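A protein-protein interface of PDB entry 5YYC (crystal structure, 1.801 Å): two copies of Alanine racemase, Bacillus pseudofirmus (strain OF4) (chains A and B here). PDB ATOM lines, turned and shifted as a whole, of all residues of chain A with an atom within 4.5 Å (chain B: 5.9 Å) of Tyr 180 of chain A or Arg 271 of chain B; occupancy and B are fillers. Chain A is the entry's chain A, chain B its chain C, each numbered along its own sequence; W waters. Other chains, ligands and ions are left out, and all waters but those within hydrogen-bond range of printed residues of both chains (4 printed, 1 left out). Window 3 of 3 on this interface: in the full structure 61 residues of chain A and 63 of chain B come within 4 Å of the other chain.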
ATOM      1  N   GLY A 136     -11.822 -12.324  16.625  1.00  0.00           N
ATOM      2  CA  GLY A 136     -12.243 -12.429  15.243  1.00  0.00           C
ATOM      3  C   GLY A 136     -13.400 -13.362  14.949  1.00  0.00           C
ATOM      4  O   GLY A 136     -13.875 -13.410  13.821  1.00  0.00           O
ATOM      5  N   ALA A 171     -12.463 -18.670  14.136  1.00  0.00           N
ATOM      6  CA  ALA A 171     -13.554 -18.734  13.160  1.00  0.00           C
ATOM      7  C   ALA A 171     -13.329 -19.708  11.997  1.00  0.00           C
ATOM      8  O   ALA A 171     -14.296 -20.199  11.405  1.00  0.00           O
ATOM      9  CB  ALA A 171     -13.826 -17.331  12.593  1.00  0.00           C
ATOM     10  N   GLU A 172     -12.075 -19.967  11.629  1.00  0.00           N
ATOM     11  CA  GLU A 172     -11.832 -20.845  10.479  1.00  0.00           C
ATOM     12  C   GLU A 172     -10.461 -21.512  10.552  1.00  0.00           C
ATOM     13  O   GLU A 172      -9.686 -21.480   9.600  1.00  0.00           O
ATOM     14  CB  GLU A 172     -11.987 -20.084   9.143  1.00  0.00           C
ATOM     15  CG  GLU A 172     -11.163 -18.786   8.991  1.00  0.00           C
ATOM     16  CD  GLU A 172     -11.393 -18.086   7.642  1.00  0.00           C
ATOM     17  OE1 GLU A 172     -10.476 -17.385   7.164  1.00  0.00           O
ATOM     18  OE2 GLU A 172     -12.487 -18.234   7.058  1.00  0.00           O
ATOM     19  N   SER A 178      -6.029 -19.996   4.826  1.00  0.00           N
ATOM     20  CA  SER A 178      -6.329 -18.694   5.400  1.00  0.00           C
ATOM     21  C   SER A 178      -5.245 -18.239   6.387  1.00  0.00           C
ATOM     22  O   SER A 178      -4.655 -19.061   7.098  1.00  0.00           O
ATOM     23  CB  SER A 178      -7.684 -18.748   6.106  1.00  0.00           C
ATOM     24  OG  SER A 178      -7.921 -17.580   6.871  1.00  0.00           O
ATOM     25  N   THR A 179      -4.990 -16.933   6.422  1.00  0.00           N
ATOM     26  CA  THR A 179      -4.120 -16.335   7.442  1.00  0.00           C
ATOM     27  C   THR A 179      -4.892 -15.968   8.706  1.00  0.00           C
ATOM     28  O   THR A 179      -4.305 -15.498   9.673  1.00  0.00           O
ATOM     29  CB  THR A 179      -3.432 -15.046   6.936  1.00  0.00           C
ATOM     30  OG1 THR A 179      -4.437 -14.120   6.506  1.00  0.00           O
ATOM     31  CG2 THR A 179      -2.485 -15.333   5.776  1.00  0.00           C
ATOM     32  N   TYR A 180      -6.211 -16.163   8.701  1.00  0.00           N
ATOM     33  CA  TYR A 180      -7.041 -15.601   9.771  1.00  0.00           C
ATOM     34  C   TYR A 180      -6.725 -16.210  11.129  1.00  0.00           C
ATOM     35  O   TYR A 180      -6.769 -15.522  12.147  1.00  0.00           O
ATOM     36  CB  TYR A 180      -8.520 -15.803   9.460  1.00  0.00           C
ATOM     37  CG  TYR A 180      -9.458 -14.871  10.208  1.00  0.00           C
ATOM     38  CD1 TYR A 180      -9.408 -13.487  10.003  1.00  0.00           C
ATOM     39  CD2 TYR A 180     -10.408 -15.371  11.090  1.00  0.00           C
ATOM     40  CE1 TYR A 180     -10.278 -12.628  10.655  1.00  0.00           C
ATOM     41  CE2 TYR A 180     -11.286 -14.517  11.752  1.00  0.00           C
ATOM     42  CZ  TYR A 180     -11.212 -13.148  11.529  1.00  0.00           C
ATOM     43  OH  TYR A 180     -12.078 -12.287  12.165  1.00  0.00           O
ATOM     44  N   THR A 181      -6.416 -17.503  11.150  1.00  0.00           N
ATOM     45  CA  THR A 181      -6.133 -18.153  12.426  1.00  0.00           C
ATOM     46  C   THR A 181      -4.840 -17.595  13.029  1.00  0.00           C
ATOM     47  O   THR A 181      -4.764 -17.347  14.234  1.00  0.00           O
ATOM     48  CB  THR A 181      -6.045 -19.683  12.268  1.00  0.00           C
ATOM     49  OG1 THR A 181      -7.284 -20.157  11.716  1.00  0.00           O
ATOM     50  CG2 THR A 181      -5.812 -20.347  13.621  1.00  0.00           C
ATOM     51  N   ASP A 182      -3.828 -17.380  12.195  1.00  0.00           N
ATOM     52  CA  ASP A 182      -2.600 -16.748  12.691  1.00  0.00           C
ATOM     53  C   ASP A 182      -2.861 -15.309  13.146  1.00  0.00           C
ATOM     54  O   ASP A 182      -2.282 -14.850  14.132  1.00  0.00           O
ATOM     55  CB  ASP A 182      -1.502 -16.794  11.625  1.00  0.00           C
ATOM     56  CG  ASP A 182      -1.021 -18.213  11.355  1.00  0.00           C
ATOM     57  OD1 ASP A 182      -0.485 -18.847  12.294  1.00  0.00           O
ATOM     58  OD2 ASP A 182      -1.181 -18.697  10.211  1.00  0.00           O
ATOM     59  N   GLU A 183      -3.731 -14.594  12.435  1.00  0.00           N
ATOM     60  CA  GLU A 183      -4.093 -13.228  12.839  1.00  0.00           C
ATOM     61  C   GLU A 183      -4.820 -13.217  14.190  1.00  0.00           C
ATOM     62  O   GLU A 183      -4.508 -12.396  15.063  1.00  0.00           O
ATOM     63  CB  GLU A 183      -4.943 -12.566  11.742  1.00  0.00           C
ATOM     64  CG  GLU A 183      -4.108 -12.304  10.486  1.00  0.00           C
ATOM     65  CD  GLU A 183      -4.926 -12.058   9.232  1.00  0.00           C
ATOM     66  OE1 GLU A 183      -6.159 -11.966   9.328  1.00  0.00           O
ATOM     67  OE2 GLU A 183      -4.323 -11.941   8.142  1.00  0.00           O
ATOM     68  N   GLN A 184      -5.764 -14.138  14.375  1.00  0.00           N
ATOM     69  CA  GLN A 184      -6.460 -14.255  15.657  1.00  0.00           C
ATOM     70  C   GLN A 184      -5.496 -14.592  16.790  1.00  0.00           C
ATOM     71  O   GLN A 184      -5.591 -14.040  17.890  1.00  0.00           O
ATOM     72  CB  GLN A 184      -7.544 -15.323  15.593  1.00  0.00           C
ATOM     73  CG  GLN A 184      -8.730 -14.983  14.687  1.00  0.00           C
ATOM     74  CD  GLN A 184      -9.924 -15.873  14.969  1.00  0.00           C
ATOM     75  OE1 GLN A 184     -10.259 -16.752  14.178  1.00  0.00           O
ATOM     76  NE2 GLN A 184     -10.573 -15.648  16.109  1.00  0.00           N
ATOM     77  N   ARG A 187      -3.568 -11.586  17.863  1.00  0.00           N
ATOM     78  CA  ARG A 187      -4.379 -10.709  18.689  1.00  0.00           C
ATOM     79  C   ARG A 187      -4.553 -11.294  20.079  1.00  0.00           C
ATOM     80  O   ARG A 187      -4.553 -10.562  21.066  1.00  0.00           O
ATOM     81  CB  ARG A 187      -5.739 -10.454  18.036  1.00  0.00           C
ATOM     82  CG  ARG A 187      -5.606  -9.650  16.745  1.00  0.00           C
ATOM     83  CD  ARG A 187      -6.944  -9.135  16.241  1.00  0.00           C
ATOM     84  NE  ARG A 187      -7.698 -10.120  15.471  1.00  0.00           N
ATOM     85  CZ  ARG A 187      -7.568 -10.316  14.160  1.00  0.00           C
ATOM     86  NH1 ARG A 187      -6.674  -9.623  13.460  1.00  0.00           N
ATOM     87  NH2 ARG A 187      -8.329 -11.217  13.549  1.00  0.00           N
ATOM     88  N   GLY B 264     -16.135  -4.118   8.207  1.00  0.00           N
ATOM     89  CA  GLY B 264     -15.156  -5.115   7.819  1.00  0.00           C
ATOM     90  C   GLY B 264     -14.995  -6.294   8.768  1.00  0.00           C
ATOM     91  O   GLY B 264     -14.402  -7.301   8.385  1.00  0.00           O
ATOM     92  N   SER B 265     -15.495  -6.179   9.997  1.00  0.00           N
ATOM     93  CA  SER B 265     -15.479  -7.306  10.938  1.00  0.00           C
ATOM     94  C   SER B 265     -16.274  -8.466  10.375  1.00  0.00           C
ATOM     95  O   SER B 265     -17.341  -8.261   9.810  1.00  0.00           O
ATOM     96  CB  SER B 265     -16.088  -6.934  12.300  1.00  0.00           C
ATOM     97  OG  SER B 265     -15.518  -5.769  12.845  1.00  0.00           O
ATOM     98  N   SER B 266     -15.786  -9.687  10.557  1.00  0.00           N
ATOM     99  CA  SER B 266     -16.565 -10.837  10.136  1.00  0.00           C
ATOM    100  C   SER B 266     -17.276 -11.456  11.335  1.00  0.00           C
ATOM    101  O   SER B 266     -16.806 -11.366  12.467  1.00  0.00           O
ATOM    102  CB  SER B 266     -15.681 -11.869   9.455  1.00  0.00           C
ATOM    103  OG  SER B 266     -14.731 -12.355  10.377  1.00  0.00           O
ATOM    104  N   ILE B 267     -18.417 -12.079  11.075  1.00  0.00           N
ATOM    105  CA  ILE B 267     -19.232 -12.653  12.136  1.00  0.00           C
ATOM    106  C   ILE B 267     -19.321 -14.157  11.950  1.00  0.00           C
ATOM    107  O   ILE B 267     -19.754 -14.638  10.890  1.00  0.00           O
ATOM    108  CB  ILE B 267     -20.671 -12.055  12.160  1.00  0.00           C
ATOM    109  CG1 ILE B 267     -20.634 -10.517  12.131  1.00  0.00           C
ATOM    110  CG2 ILE B 267     -21.458 -12.573  13.365  1.00  0.00           C
ATOM    111  CD1 ILE B 267     -19.937  -9.887  13.342  1.00  0.00           C
ATOM    112  N   SER B 268     -18.876 -14.872  12.983  1.00  0.00           N
ATOM    113  CA  SER B 268     -19.058 -16.312  13.163  1.00  0.00           C
ATOM    114  C   SER B 268     -18.230 -17.168  12.210  1.00  0.00           C
ATOM    115  O   SER B 268     -17.372 -16.666  11.487  1.00  0.00           O
ATOM    116  CB  SER B 268     -20.540 -16.692  13.038  1.00  0.00           C
ATOM    117  OG  SER B 268     -20.764 -17.956  13.650  1.00  0.00           O
ATOM    118  N   TYR B 269     -18.479 -18.475  12.239  1.00  0.00           N
ATOM    119  CA  TYR B 269     -17.623 -19.429  11.529  1.00  0.00           C
ATOM    120  C   TYR B 269     -17.542 -19.168  10.038  1.00  0.00           C
ATOM    121  O   TYR B 269     -18.541 -18.832   9.414  1.00  0.00           O
ATOM    122  CB  TYR B 269     -18.122 -20.855  11.732  1.00  0.00           C
ATOM    123  CG  TYR B 269     -17.929 -21.401  13.120  1.00  0.00           C
ATOM    124  CD1 TYR B 269     -16.652 -21.596  13.639  1.00  0.00           C
ATOM    125  CD2 TYR B 269     -19.019 -21.762  13.895  1.00  0.00           C
ATOM    126  CE1 TYR B 269     -16.471 -22.114  14.901  1.00  0.00           C
ATOM    127  CE2 TYR B 269     -18.850 -22.286  15.164  1.00  0.00           C
ATOM    128  CZ  TYR B 269     -17.577 -22.463  15.655  1.00  0.00           C
ATOM    129  OH  TYR B 269     -17.436 -23.002  16.905  1.00  0.00           O
ATOM    130  N   GLY B 270     -16.358 -19.364   9.464  1.00  0.00           N
ATOM    131  CA  GLY B 270     -16.177 -19.215   8.028  1.00  0.00           C
ATOM    132  C   GLY B 270     -16.237 -17.781   7.524  1.00  0.00           C
ATOM    133  O   GLY B 270     -16.160 -17.547   6.317  1.00  0.00           O
ATOM    134  N   ARG B 271     -16.380 -16.822   8.440  1.00  0.00           N
ATOM    135  CA  ARG B 271     -16.447 -15.403   8.079  1.00  0.00           C
ATOM    136  C   ARG B 271     -17.473 -15.135   6.981  1.00  0.00           C
ATOM    137  O   ARG B 271     -17.195 -14.385   6.038  1.00  0.00           O
ATOM    138  CB  ARG B 271     -15.071 -14.906   7.622  1.00  0.00           C
ATOM    139  CG  ARG B 271     -13.961 -15.317   8.558  1.00  0.00           C
ATOM    140  CD  ARG B 271     -13.055 -14.151   8.838  1.00  0.00           C
ATOM    141  NE  ARG B 271     -12.053 -13.955   7.817  1.00  0.00           N
ATOM    142  CZ  ARG B 271     -11.559 -12.775   7.455  1.00  0.00           C
ATOM    143  NH1 ARG B 271     -11.986 -11.648   8.012  1.00  0.00           N
ATOM    144  NH2 ARG B 271     -10.627 -12.731   6.526  1.00  0.00           N
ATOM    145  N   THR B 272     -18.644 -15.757   7.084  1.00  0.00           N
ATOM    146  CA  THR B 272     -19.586 -15.738   5.963  1.00  0.00           C
ATOM    147  C   THR B 272     -20.328 -14.415   5.866  1.00  0.00           C
ATOM    148  O   THR B 272     -20.986 -14.144   4.865  1.00  0.00           O
ATOM    149  CB  THR B 272     -20.623 -16.871   6.061  1.00  0.00           C
ATOM    150  OG1 THR B 272     -21.516 -16.620   7.155  1.00  0.00           O
ATOM    151  CG2 THR B 272     -19.934 -18.221   6.242  1.00  0.00           C
ATOM    152  N   HIS B 273     -20.241 -13.606   6.916  1.00  0.00           N
ATOM    153  CA  HIS B 273     -20.798 -12.257   6.880  1.00  0.00           C
ATOM    154  C   HIS B 273     -19.752 -11.252   7.327  1.00  0.00           C
ATOM    155  O   HIS B 273     -19.136 -11.429   8.376  1.00  0.00           O
ATOM    156  CB  HIS B 273     -22.031 -12.133   7.781  1.00  0.00           C
ATOM    157  CG  HIS B 273     -22.645 -10.768   7.755  1.00  0.00           C
ATOM    158  ND1 HIS B 273     -23.549 -10.380   6.790  1.00  0.00           N
ATOM    159  CD2 HIS B 273     -22.463  -9.690   8.553  1.00  0.00           C
ATOM    160  CE1 HIS B 273     -23.905  -9.124   6.999  1.00  0.00           C
ATOM    161  NE2 HIS B 273     -23.259  -8.680   8.062  1.00  0.00           N
ATOM    162  N   LYS B 274     -19.552 -10.202   6.536  1.00  0.00           N
ATOM    163  CA  LYS B 274     -18.672  -9.107   6.938  1.00  0.00           C
ATOM    164  C   LYS B 274     -19.475  -7.813   7.017  1.00  0.00           C
ATOM    165  O   LYS B 274     -20.249  -7.509   6.113  1.00  0.00           O
ATOM    166  CB  LYS B 274     -17.497  -8.970   5.968  1.00  0.00           C
ATOM    167  CG  LYS B 274     -16.578 -10.181   5.999  1.00  0.00           C
ATOM    168  CD  LYS B 274     -15.311  -9.976   5.186  1.00  0.00           C
ATOM    169  CE  LYS B 274     -14.533 -11.291   5.086  1.00  0.00           C
ATOM    170  NZ  LYS B 274     -13.451 -11.234   4.057  1.00  0.00           N
HETATM  171  O   HOH W   1      -7.675 -11.981   6.903  1.00  0.00           O
HETATM  172  O   HOH W   2     -12.891  -9.890  10.647  1.00  0.00           O
HETATM  173  O   HOH W   3     -10.424 -15.398   5.550  1.00  0.00           O
HETATM  174  O   HOH W   4     -15.591 -14.338  11.713  1.00  0.00           O
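N of Gly 270 of chain B is in hydrogen-bond range of O of Ala 171 of chain A (3.0 Å).
The guanidinium group (NE) of Arg 271 of chain B is in salt-bridge range of the side-chain carboxylate (OE1) of Glu 172 of chain A, 3.8 Å away.
OG of Ser 266 of chain B is in hydrogen-bond range of OH of Tyr 180 of chain A (3.2 Å).
OH of Tyr 180 of chain A lies within hydrogen-bond range of O of Gly 136 of chain A (2.7 Å).
The backbone NH (N) of Ala 171 of chain A is in hydrogen-bond range of the side-chain amide oxygen (OE1) of Gln 184 of chain A, at 2.9 Å.
The side-chain hydroxyl (OG) of Ser 178 of chain A is in hydrogen-bond range of the side-chain carboxylate (OE1) of Glu 172 of chain A, at 2.6 Å.
The backbone carbonyl oxygen (O) of Glu 172 of chain A sits at hydrogen-bond distance from the side-chain hydroxyl (OG1) of Thr 181 of chain A (3.5 Å).
OG of Ser 178 of chain A is in hydrogen-bond range of N of Tyr 180 of chain A (2.9 Å).
Among the printed residues, merely in contact across the chains: Gly 136 of chain A with Ser 266 of chain B, Ala 171 of chain A with Ser 268 of chain B, Ala 171 of chain A with Tyr 269 of chain B, Glu 172 of chain A with Gly 270 of chain B and Tyr 180 of chain A with Arg 271 of chain B.
Of the printed residues of chain B, Gly 136 of chain A touches Ser 266.
Of chain B, only Ser 266 and Arg 271 come within 4 Å of Tyr 180 of chain A.
Of the printed residues of chain A, Ser 266 of chain B touches Gly 136 and Tyr 180.
Of the printed residues of chain A, Ser 268 of chain B touches Ala 171 (3.8 Å).
Of the printed residues of chain A, Gly 270 of chain B touches Ala 171 (3.0 Å) and Glu 172 (3.8 Å).
The nearest printed residue of chain A that does not touch Arg 271 of chain B is Ala 171 of chain A (4.5 Å).
Printed residues of chain B that touch a printed residue of chain A: Ser 266, Ser 268, Tyr 269, Gly 270 and Arg 271.
Hydrophobic or aromatic side chains of chain B within 4 Å of the printed part of chain A: Tyr 269.
Printed residues of chain A that touch a printed residue of chain B: Gly 136, Ala 171, Glu 172 and Tyr 180.
Hydrophobic or aromatic side chains of chain A within 4 Å of the printed part of chain B: Ala 171 and Tyr 180.
Along chain A the printed residues that touch a printed residue of chain B span positions 136 to 180.
Among the printed residues, 8 pairs touch across the chains.
Among the printed residues, Asp or Glu carboxylates within 4 Å of a Lys or Arg side-chain nitrogen of the other chain: Glu 172 of chain A with Arg 271 of chain B.
No position is printed for both chains.
Water W4 lies within hydrogen-bond range of the side-chain hydroxyl (OG) of Ser 266 of chain B (2.5 Å), the backbone carbonyl oxygen (O) of Gly 136 of chain A (2.9 Å) and the backbone carbonyl oxygen (O) of Ser 268 of chain B (2.9 Å).
Water W3 lies within hydrogen-bond range of OE1 of Glu 172 of chain A (2.6 Å) and NH2 of Arg 271 of chain B (2.8 Å).
Water W1 lies within hydrogen-bond range of OE1 of Glu 183 of chain A and NH2 of Arg 271 of chain B.
Water W2 lies within hydrogen-bond range of N of Ser 266 of chain B (2.9 Å), OH of Tyr 180 of chain A (3.0 Å) and NH1 of Arg 271 of chain B (3.3 Å).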
